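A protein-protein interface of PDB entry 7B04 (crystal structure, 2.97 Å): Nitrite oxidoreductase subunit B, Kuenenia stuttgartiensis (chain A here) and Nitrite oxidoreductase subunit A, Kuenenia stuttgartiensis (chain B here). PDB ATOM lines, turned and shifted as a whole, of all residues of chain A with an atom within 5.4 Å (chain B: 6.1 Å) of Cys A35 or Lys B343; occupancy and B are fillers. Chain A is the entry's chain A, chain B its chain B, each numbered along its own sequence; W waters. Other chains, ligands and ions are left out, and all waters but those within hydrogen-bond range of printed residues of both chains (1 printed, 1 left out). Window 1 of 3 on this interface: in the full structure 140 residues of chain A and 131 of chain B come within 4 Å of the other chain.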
ATOM      1  N   ASN A  31      18.019 -21.589  10.310  1.00  0.00           N
ATOM      2  CA  ASN A  31      17.576 -20.209  10.520  1.00  0.00           C
ATOM      3  C   ASN A  31      18.815 -19.323  10.507  1.00  0.00           C
ATOM      4  O   ASN A  31      19.471 -19.121  11.530  1.00  0.00           O
ATOM      5  CB  ASN A  31      16.793 -20.079  11.821  1.00  0.00           C
ATOM      6  CG  ASN A  31      16.086 -18.741  11.944  1.00  0.00           C
ATOM      7  OD1 ASN A  31      16.213 -17.875  11.078  1.00  0.00           O
ATOM      8  ND2 ASN A  31      15.336 -18.567  13.025  1.00  0.00           N
ATOM      9  N   ILE A  32      19.132 -18.780   9.328  1.00  0.00           N
ATOM     10  CA  ILE A  32      20.319 -17.941   9.170  1.00  0.00           C
ATOM     11  C   ILE A  32      20.270 -16.734  10.099  1.00  0.00           C
ATOM     12  O   ILE A  32      21.310 -16.259  10.571  1.00  0.00           O
ATOM     13  CB  ILE A  32      20.472 -17.508   7.698  1.00  0.00           C
ATOM     14  CG1 ILE A  32      20.541 -18.730   6.782  1.00  0.00           C
ATOM     15  CG2 ILE A  32      21.712 -16.651   7.514  1.00  0.00           C
ATOM     16  CD1 ILE A  32      20.606 -18.373   5.313  1.00  0.00           C
ATOM     17  N   ASN A  33      19.068 -16.227  10.382  1.00  0.00           N
ATOM     18  CA  ASN A  33      18.927 -15.056  11.243  1.00  0.00           C
ATOM     19  C   ASN A  33      19.537 -15.273  12.622  1.00  0.00           C
ATOM     20  O   ASN A  33      19.962 -14.308  13.266  1.00  0.00           O
ATOM     21  CB  ASN A  33      17.452 -14.687  11.371  1.00  0.00           C
ATOM     22  CG  ASN A  33      16.848 -14.243  10.055  1.00  0.00           C
ATOM     23  OD1 ASN A  33      17.294 -13.266   9.454  1.00  0.00           O
ATOM     24  ND2 ASN A  33      15.830 -14.962   9.596  1.00  0.00           N
ATOM     25  N   ARG A  34      19.580 -16.515  13.098  1.00  0.00           N
ATOM     26  CA  ARG A  34      20.109 -16.808  14.425  1.00  0.00           C
ATOM     27  C   ARG A  34      21.584 -17.191  14.423  1.00  0.00           C
ATOM     28  O   ARG A  34      22.164 -17.341  15.504  1.00  0.00           O
ATOM     29  CB  ARG A  34      19.320 -17.947  15.077  1.00  0.00           C
ATOM     30  CG  ARG A  34      17.884 -17.652  15.449  1.00  0.00           C
ATOM     31  CD  ARG A  34      17.317 -18.861  16.175  1.00  0.00           C
ATOM     32  NE  ARG A  34      15.924 -18.702  16.574  1.00  0.00           N
ATOM     33  CZ  ARG A  34      15.235 -19.623  17.240  1.00  0.00           C
ATOM     34  NH1 ARG A  34      13.970 -19.402  17.565  1.00  0.00           N
ATOM     35  NH2 ARG A  34      15.816 -20.766  17.582  1.00  0.00           N
ATOM     36  N   CYS A  35      22.205 -17.354  13.258  1.00  0.00           N
ATOM     37  CA  CYS A  35      23.550 -17.912  13.212  1.00  0.00           C
ATOM     38  C   CYS A  35      24.587 -16.909  13.706  1.00  0.00           C
ATOM     39  O   CYS A  35      24.426 -15.693  13.582  1.00  0.00           O
ATOM     40  CB  CYS A  35      23.897 -18.355  11.791  1.00  0.00           C
ATOM     41  SG  CYS A  35      25.422 -19.327  11.664  1.00  0.00           S
ATOM     42  N   ILE A  36      25.673 -17.445  14.259  1.00  0.00           N
ATOM     43  CA  ILE A  36      26.746 -16.655  14.848  1.00  0.00           C
ATOM     44  C   ILE A  36      28.096 -16.936  14.208  1.00  0.00           C
ATOM     45  O   ILE A  36      29.091 -16.313  14.594  1.00  0.00           O
ATOM     46  CB  ILE A  36      26.823 -16.871  16.374  1.00  0.00           C
ATOM     47  CG1 ILE A  36      27.033 -18.351  16.690  1.00  0.00           C
ATOM     48  CG2 ILE A  36      25.558 -16.363  17.048  1.00  0.00           C
ATOM     49  CD1 ILE A  36      27.062 -18.657  18.167  1.00  0.00           C
ATOM     50  N   ALA A  37      28.161 -17.868  13.254  1.00  0.00           N
ATOM     51  CA  ALA A  37      29.409 -18.302  12.622  1.00  0.00           C
ATOM     52  C   ALA A  37      30.410 -18.845  13.634  1.00  0.00           C
ATOM     53  O   ALA A  37      31.623 -18.705  13.458  1.00  0.00           O
ATOM     54  CB  ALA A  37      30.047 -17.180  11.800  1.00  0.00           C
ATOM     55  N   VAL A  63      30.976 -23.110   7.583  1.00  0.00           N
ATOM     56  CA  VAL A  63      30.092 -21.920   7.614  1.00  0.00           C
ATOM     57  C   VAL A  63      30.934 -20.803   7.022  1.00  0.00           C
ATOM     58  O   VAL A  63      32.010 -20.587   7.484  1.00  0.00           O
ATOM     59  CB  VAL A  63      29.613 -21.596   9.030  1.00  0.00           C
ATOM     60  CG1 VAL A  63      28.666 -20.431   9.028  1.00  0.00           C
ATOM     61  CG2 VAL A  63      28.943 -22.791   9.632  1.00  0.00           C
ATOM     62  N   HIS A 164      20.469  -3.732   4.696  1.00  0.00           N
ATOM     63  CA  HIS A 164      21.662  -3.073   5.214  1.00  0.00           C
ATOM     64  C   HIS A 164      22.556  -2.659   4.048  1.00  0.00           C
ATOM     65  O   HIS A 164      22.910  -3.485   3.199  1.00  0.00           O
ATOM     66  CB  HIS A 164      22.440  -4.007   6.134  1.00  0.00           C
ATOM     67  CG  HIS A 164      21.746  -4.325   7.426  1.00  0.00           C
ATOM     68  ND1 HIS A 164      22.350  -5.077   8.414  1.00  0.00           N
ATOM     69  CD2 HIS A 164      20.515  -4.000   7.894  1.00  0.00           C
ATOM     70  CE1 HIS A 164      21.525  -5.196   9.437  1.00  0.00           C
ATOM     71  NE2 HIS A 164      20.406  -4.553   9.147  1.00  0.00           N
ATOM     72  N   TYR A 170      25.875 -15.299   7.077  1.00  0.00           N
ATOM     73  CA  TYR A 170      26.577 -16.566   7.220  1.00  0.00           C
ATOM     74  C   TYR A 170      25.806 -17.671   6.514  1.00  0.00           C
ATOM     75  O   TYR A 170      24.586 -17.781   6.672  1.00  0.00           O
ATOM     76  CB  TYR A 170      26.776 -16.912   8.696  1.00  0.00           C
ATOM     77  CG  TYR A 170      27.588 -15.887   9.453  1.00  0.00           C
ATOM     78  CD1 TYR A 170      28.815 -15.453   8.968  1.00  0.00           C
ATOM     79  CD2 TYR A 170      27.129 -15.354  10.651  1.00  0.00           C
ATOM     80  CE1 TYR A 170      29.562 -14.516   9.654  1.00  0.00           C
ATOM     81  CE2 TYR A 170      27.871 -14.416  11.345  1.00  0.00           C
ATOM     82  CZ  TYR A 170      29.087 -14.002  10.841  1.00  0.00           C
ATOM     83  OH  TYR A 170      29.834 -13.073  11.522  1.00  0.00           O
ATOM     84  N   GLN A 172      25.704 -21.778   6.097  1.00  0.00           N
ATOM     85  CA  GLN A 172      26.127 -23.012   6.748  1.00  0.00           C
ATOM     86  C   GLN A 172      25.825 -24.181   5.820  1.00  0.00           C
ATOM     87  O   GLN A 172      24.656 -24.457   5.530  1.00  0.00           O
ATOM     88  CB  GLN A 172      25.421 -23.188   8.092  1.00  0.00           C
ATOM     89  CG  GLN A 172      25.323 -21.912   8.917  1.00  0.00           C
ATOM     90  CD  GLN A 172      24.150 -21.039   8.511  1.00  0.00           C
ATOM     91  OE1 GLN A 172      23.221 -21.497   7.844  1.00  0.00           O
ATOM     92  NE2 GLN A 172      24.194 -19.771   8.899  1.00  0.00           N
ATOM     93  N   GLY A 264      23.665 -21.562  18.218  1.00  0.00           N
ATOM     94  CA  GLY A 264      22.685 -20.499  18.155  1.00  0.00           C
ATOM     95  C   GLY A 264      21.298 -20.988  17.797  1.00  0.00           C
ATOM     96  O   GLY A 264      20.462 -20.203  17.337  1.00  0.00           O
ATOM     97  N   ILE A 266      19.880 -22.707  15.424  1.00  0.00           N
ATOM     98  CA  ILE A 266      19.401 -22.309  14.104  1.00  0.00           C
ATOM     99  C   ILE A 266      18.954 -23.475  13.223  1.00  0.00           C
ATOM    100  O   ILE A 266      18.181 -23.255  12.279  1.00  0.00           O
ATOM    101  CB  ILE A 266      20.476 -21.488  13.358  1.00  0.00           C
ATOM    102  CG1 ILE A 266      21.430 -22.406  12.596  1.00  0.00           C
ATOM    103  CG2 ILE A 266      21.271 -20.640  14.321  1.00  0.00           C
ATOM    104  CD1 ILE A 266      22.186 -21.710  11.490  1.00  0.00           C
ATOM    105  N   ARG A 309      16.981 -11.415   7.307  1.00  0.00           N
ATOM    106  CA  ARG A 309      16.047 -10.298   7.203  1.00  0.00           C
ATOM    107  C   ARG A 309      16.704  -9.029   6.674  1.00  0.00           C
ATOM    108  O   ARG A 309      15.996  -8.128   6.212  1.00  0.00           O
ATOM    109  CB  ARG A 309      15.404 -10.024   8.563  1.00  0.00           C
ATOM    110  CG  ARG A 309      16.368  -9.499   9.609  1.00  0.00           C
ATOM    111  CD  ARG A 309      15.634  -9.023  10.849  1.00  0.00           C
ATOM    112  NE  ARG A 309      16.548  -8.440  11.826  1.00  0.00           N
ATOM    113  CZ  ARG A 309      16.160  -7.786  12.916  1.00  0.00           C
ATOM    114  NH1 ARG A 309      17.063  -7.290  13.749  1.00  0.00           N
ATOM    115  NH2 ARG A 309      14.868  -7.629  13.172  1.00  0.00           N
ATOM    116  N   TRP A 310      18.032  -8.934   6.733  1.00  0.00           N
ATOM    117  CA  TRP A 310      18.736  -7.680   6.511  1.00  0.00           C
ATOM    118  C   TRP A 310      19.515  -7.632   5.205  1.00  0.00           C
ATOM    119  O   TRP A 310      19.979  -6.551   4.825  1.00  0.00           O
ATOM    120  CB  TRP A 310      19.710  -7.420   7.667  1.00  0.00           C
ATOM    121  CG  TRP A 310      20.807  -8.435   7.729  1.00  0.00           C
ATOM    122  CD1 TRP A 310      22.038  -8.349   7.147  1.00  0.00           C
ATOM    123  CD2 TRP A 310      20.765  -9.700   8.397  1.00  0.00           C
ATOM    124  NE1 TRP A 310      22.768  -9.480   7.418  1.00  0.00           N
ATOM    125  CE2 TRP A 310      22.009 -10.325   8.184  1.00  0.00           C
ATOM    126  CE3 TRP A 310      19.798 -10.363   9.158  1.00  0.00           C
ATOM    127  CZ2 TRP A 310      22.310 -11.581   8.706  1.00  0.00           C
ATOM    128  CZ3 TRP A 310      20.099 -11.609   9.674  1.00  0.00           C
ATOM    129  CH2 TRP A 310      21.345 -12.205   9.446  1.00  0.00           C
ATOM    130  N   ILE B 310      27.628 -11.672  19.743  1.00  0.00           N
ATOM    131  CA  ILE B 310      27.669 -12.794  18.769  1.00  0.00           C
ATOM    132  C   ILE B 310      29.010 -13.519  18.783  1.00  0.00           C
ATOM    133  O   ILE B 310      28.975 -14.705  18.596  1.00  0.00           O
ATOM    134  CB  ILE B 310      27.320 -12.279  17.373  1.00  0.00           C
ATOM    135  CG1 ILE B 310      25.822 -12.059  17.226  1.00  0.00           C
ATOM    136  CG2 ILE B 310      27.836 -13.231  16.331  1.00  0.00           C
ATOM    137  CD1 ILE B 310      25.166 -11.732  18.504  1.00  0.00           C
ATOM    138  N   VAL B 320      19.966 -13.240  22.559  1.00  0.00           N
ATOM    139  CA  VAL B 320      19.837 -11.935  21.906  1.00  0.00           C
ATOM    140  C   VAL B 320      19.333 -12.065  20.474  1.00  0.00           C
ATOM    141  O   VAL B 320      18.476 -11.287  20.047  1.00  0.00           O
ATOM    142  CB  VAL B 320      21.150 -11.117  21.972  1.00  0.00           C
ATOM    143  CG1 VAL B 320      22.255 -11.722  21.149  1.00  0.00           C
ATOM    144  CG2 VAL B 320      20.896  -9.732  21.442  1.00  0.00           C
ATOM    145  N   THR B 321      19.862 -13.024  19.707  1.00  0.00           N
ATOM    146  CA  THR B 321      19.429 -13.194  18.323  1.00  0.00           C
ATOM    147  C   THR B 321      17.927 -13.409  18.232  1.00  0.00           C
ATOM    148  O   THR B 321      17.308 -13.053  17.222  1.00  0.00           O
ATOM    149  CB  THR B 321      20.166 -14.367  17.671  1.00  0.00           C
ATOM    150  OG1 THR B 321      19.834 -15.583  18.355  1.00  0.00           O
ATOM    151  CG2 THR B 321      21.668 -14.152  17.723  1.00  0.00           C
ATOM    152  N   MET B 324      14.747 -10.427  17.960  1.00  0.00           N
ATOM    153  CA  MET B 324      14.081 -10.036  16.725  1.00  0.00           C
ATOM    154  C   MET B 324      12.909 -10.943  16.382  1.00  0.00           C
ATOM    155  O   MET B 324      12.241 -10.699  15.373  1.00  0.00           O
ATOM    156  CB  MET B 324      15.082 -10.031  15.564  1.00  0.00           C
ATOM    157  CG  MET B 324      15.507 -11.419  15.122  1.00  0.00           C
ATOM    158  SD  MET B 324      16.580 -11.391  13.677  1.00  0.00           S
ATOM    159  CE  MET B 324      18.097 -10.781  14.404  1.00  0.00           C
ATOM    160  N   ILE B 330      16.707  -4.515  18.125  1.00  0.00           N
ATOM    161  CA  ILE B 330      18.121  -4.672  18.444  1.00  0.00           C
ATOM    162  C   ILE B 330      18.889  -3.500  17.847  1.00  0.00           C
ATOM    163  O   ILE B 330      18.653  -3.116  16.696  1.00  0.00           O
ATOM    164  CB  ILE B 330      18.669  -6.016  17.923  1.00  0.00           C
ATOM    165  CG1 ILE B 330      17.915  -7.179  18.570  1.00  0.00           C
ATOM    166  CG2 ILE B 330      20.162  -6.135  18.192  1.00  0.00           C
ATOM    167  CD1 ILE B 330      18.179  -8.518  17.921  1.00  0.00           C
ATOM    168  N   VAL B 331      19.804  -2.930  18.631  1.00  0.00           N
ATOM    169  CA  VAL B 331      20.617  -1.798  18.203  1.00  0.00           C
ATOM    170  C   VAL B 331      22.078  -2.093  18.514  1.00  0.00           C
ATOM    171  O   VAL B 331      22.401  -2.560  19.613  1.00  0.00           O
ATOM    172  CB  VAL B 331      20.185  -0.490  18.894  1.00  0.00           C
ATOM    173  CG1 VAL B 331      21.020   0.683  18.392  1.00  0.00           C
ATOM    174  CG2 VAL B 331      18.707  -0.232  18.679  1.00  0.00           C
ATOM    175  N   VAL B 332      22.955  -1.821  17.550  1.00  0.00           N
ATOM    176  CA  VAL B 332      24.395  -1.983  17.710  1.00  0.00           C
ATOM    177  C   VAL B 332      25.059  -0.665  17.339  1.00  0.00           C
ATOM    178  O   VAL B 332      24.782  -0.105  16.272  1.00  0.00           O
ATOM    179  CB  VAL B 332      24.946  -3.133  16.843  1.00  0.00           C
ATOM    180  CG1 VAL B 332      26.462  -3.190  16.934  1.00  0.00           C
ATOM    181  CG2 VAL B 332      24.334  -4.456  17.273  1.00  0.00           C
ATOM    182  N   TYR B 337      31.061  -2.653  11.049  1.00  0.00           N
ATOM    183  CA  TYR B 337      29.884  -3.493  10.848  1.00  0.00           C
ATOM    184  C   TYR B 337      30.272  -4.883  11.335  1.00  0.00           C
ATOM    185  O   TYR B 337      30.788  -5.711  10.583  1.00  0.00           O
ATOM    186  CB  TYR B 337      29.435  -3.490   9.393  1.00  0.00           C
ATOM    187  CG  TYR B 337      28.112  -4.193   9.182  1.00  0.00           C
ATOM    188  CD1 TYR B 337      26.917  -3.596   9.562  1.00  0.00           C
ATOM    189  CD2 TYR B 337      28.060  -5.457   8.614  1.00  0.00           C
ATOM    190  CE1 TYR B 337      25.706  -4.239   9.378  1.00  0.00           C
ATOM    191  CE2 TYR B 337      26.855  -6.107   8.425  1.00  0.00           C
ATOM    192  CZ  TYR B 337      25.682  -5.495   8.807  1.00  0.00           C
ATOM    193  OH  TYR B 337      24.484  -6.144   8.616  1.00  0.00           O
ATOM    194  N   PRO B 339      29.855  -8.705  13.402  1.00  0.00           N
ATOM    195  CA  PRO B 339      28.872  -9.800  13.366  1.00  0.00           C
ATOM    196  C   PRO B 339      27.662  -9.562  14.245  1.00  0.00           C
ATOM    197  O   PRO B 339      26.611 -10.167  14.004  1.00  0.00           O
ATOM    198  CB  PRO B 339      29.682 -11.008  13.843  1.00  0.00           C
ATOM    199  CG  PRO B 339      31.050 -10.703  13.381  1.00  0.00           C
ATOM    200  CD  PRO B 339      31.224  -9.220  13.576  1.00  0.00           C
ATOM    201  N   SER B 340      27.771  -8.700  15.257  1.00  0.00           N
ATOM    202  CA  SER B 340      26.605  -8.327  16.040  1.00  0.00           C
ATOM    203  C   SER B 340      25.727  -7.325  15.308  1.00  0.00           C
ATOM    204  O   SER B 340      24.538  -7.214  15.621  1.00  0.00           O
ATOM    205  CB  SER B 340      27.034  -7.753  17.390  1.00  0.00           C
ATOM    206  OG  SER B 340      27.718  -8.724  18.162  1.00  0.00           O
ATOM    207  N   ALA B 341      26.286  -6.606  14.333  1.00  0.00           N
ATOM    208  CA  ALA B 341      25.513  -5.600  13.614  1.00  0.00           C
ATOM    209  C   ALA B 341      24.502  -6.234  12.666  1.00  0.00           C
ATOM    210  O   ALA B 341      23.490  -5.603  12.340  1.00  0.00           O
ATOM    211  CB  ALA B 341      26.447  -4.663  12.855  1.00  0.00           C
ATOM    212  N   GLN B 342      24.757  -7.466  12.207  1.00  0.00           N
ATOM    213  CA  GLN B 342      23.794  -8.154  11.348  1.00  0.00           C
ATOM    214  C   GLN B 342      22.430  -8.221  12.011  1.00  0.00           C
ATOM    215  O   GLN B 342      21.398  -7.928  11.397  1.00  0.00           O
ATOM    216  CB  GLN B 342      24.230  -9.588  11.080  1.00  0.00           C
ATOM    217  CG  GLN B 342      25.531  -9.854  10.405  1.00  0.00           C
ATOM    218  CD  GLN B 342      25.774 -11.349  10.366  1.00  0.00           C
ATOM    219  OE1 GLN B 342      24.944 -12.126  10.843  1.00  0.00           O
ATOM    220  NE2 GLN B 342      26.891 -11.763   9.796  1.00  0.00           N
ATOM    221  N   LYS B 343      22.420  -8.602  13.286  1.00  0.00           N
ATOM    222  CA  LYS B 343      21.191  -8.835  14.020  1.00  0.00           C
ATOM    223  C   LYS B 343      20.498  -7.540  14.403  1.00  0.00           C
ATOM    224  O   LYS B 343      19.333  -7.578  14.813  1.00  0.00           O
ATOM    225  CB  LYS B 343      21.496  -9.667  15.265  1.00  0.00           C
ATOM    226  CG  LYS B 343      22.485 -10.808  15.026  1.00  0.00           C
ATOM    227  CD  LYS B 343      21.981 -11.766  13.955  1.00  0.00           C
ATOM    228  CE  LYS B 343      22.740 -13.082  13.980  1.00  0.00           C
ATOM    229  NZ  LYS B 343      24.035 -13.018  13.252  1.00  0.00           N
ATOM    230  N   ALA B 344      21.181  -6.407  14.269  1.00  0.00           N
ATOM    231  CA  ALA B 344      20.616  -5.134  14.686  1.00  0.00           C
ATOM    232  C   ALA B 344      19.517  -4.684  13.734  1.00  0.00           C
ATOM    233  O   ALA B 344      19.583  -4.912  12.522  1.00  0.00           O
ATOM    234  CB  ALA B 344      21.712  -4.071  14.752  1.00  0.00           C
ATOM    235  N   ASP B 345      18.498  -4.036  14.302  1.00  0.00           N
ATOM    236  CA  ASP B 345      17.475  -3.391  13.489  1.00  0.00           C
ATOM    237  C   ASP B 345      18.052  -2.207  12.726  1.00  0.00           C
ATOM    238  O   ASP B 345      17.637  -1.934  11.593  1.00  0.00           O
ATOM    239  CB  ASP B 345      16.317  -2.941  14.382  1.00  0.00           C
ATOM    240  CG  ASP B 345      15.266  -4.021  14.569  1.00  0.00           C
ATOM    241  OD1 ASP B 345      14.359  -4.131  13.720  1.00  0.00           O
ATOM    242  OD2 ASP B 345      15.358  -4.771  15.561  1.00  0.00           O
HETATM  243  O   HOH W   1      30.166 -16.577  16.804  1.00  0.00           O
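O of Cys A35 lies within hydrogen-bond range of NZ of Lys B343.
A ring nitrogen (NE2) of His A164 is in hydrogen-bond range of the backbone carbonyl oxygen (O) of Ala B344, 3.5 Å away.
NE of Arg A309 sits at hydrogen-bond distance from SD of Met B324, 3.5 Å away.
NH1 of Arg A309 lies within hydrogen-bond range of O of Lys B343, at 2.5 Å.
The side-chain carboxylate of Asp B345 is in salt-bridge range of the guanidinium group of Arg A309 (3.5 Å).
ND1 of His A164 sits close to OH of Tyr B337, 2.4 Å away.
OD1 of Asn A31 is in hydrogen-bond range of ND2 of Asn A33 (3.3 Å).
The side-chain amide oxygen of Asn A33 sits at hydrogen-bond distance from the backbone NH of Arg A309.
SG of Cys A35 lies close to NE2 of Gln A172 (3.1 Å).
The backbone NH (N) of His A164 lies within hydrogen-bond range of the backbone carbonyl oxygen (O) of Trp A310.
O of Ile B330 is in hydrogen-bond range of N of Asp B345 (2.6 Å).
OE1 of Gln B342 sits at hydrogen-bond distance from NZ of Lys B343 (2.7 Å).
Among the printed residues, merely in contact across the chains: Tyr A170 with Pro B339 (3.1 Å), Asn A33 with Lys B343 (3.1 Å), Tyr A170 with Gln B342 (3.2 Å), His A164 with Gln B342 (3.4 Å), Trp A310 with Gln B342 (3.4 Å), His A164 with Ala B341 (3.5 Å), Arg A309 with Ala B344 (3.6 Å), Trp A310 with Tyr B337 (3.6 Å), Ile A36 with Ile B310 (3.8 Å) and Arg A34 with Thr B321 (3.9 Å).
Cys A35 touches one residue of chain B.
Of the printed residues of chain A, Lys B343 touches Asn A33 (3.1 Å), Cys A35 (2.7 Å) and Arg A309 (2.5 Å).
Printed residues of chain A within 4 Å of Asp B345: Arg A309 (3.5 Å).
Printed residues of chain A within 4 Å of Gln B342: His A164 (3.4 Å), Tyr A170 (3.2 Å) and Trp A310 (3.4 Å).
The nearest residue of chain B that does not touch Cys A35 is Gln B342 (4.5 Å).
Hydrophobic or aromatic side chains of chain B that line the printed part of chain A: Ile B310, Met B324, Tyr B337 and Pro B339.
Hydrophobic or aromatic side chains of chain A within 4 Å of the printed part of chain B: Ile A36, His A164, Tyr A170 and Trp A310.
Along chain A the printed residues that touch a printed residue of chain B span positions 33 to 310.
Among the printed residues, Asp or Glu carboxylates within 4 Å of a Lys or Arg side-chain nitrogen of the other chain: Arg A309 with Asp B345.
Water W1 bridges the backbone carbonyl oxygen (O) of Ile A36 and the backbone carbonyl oxygen (O) of Ile B310.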
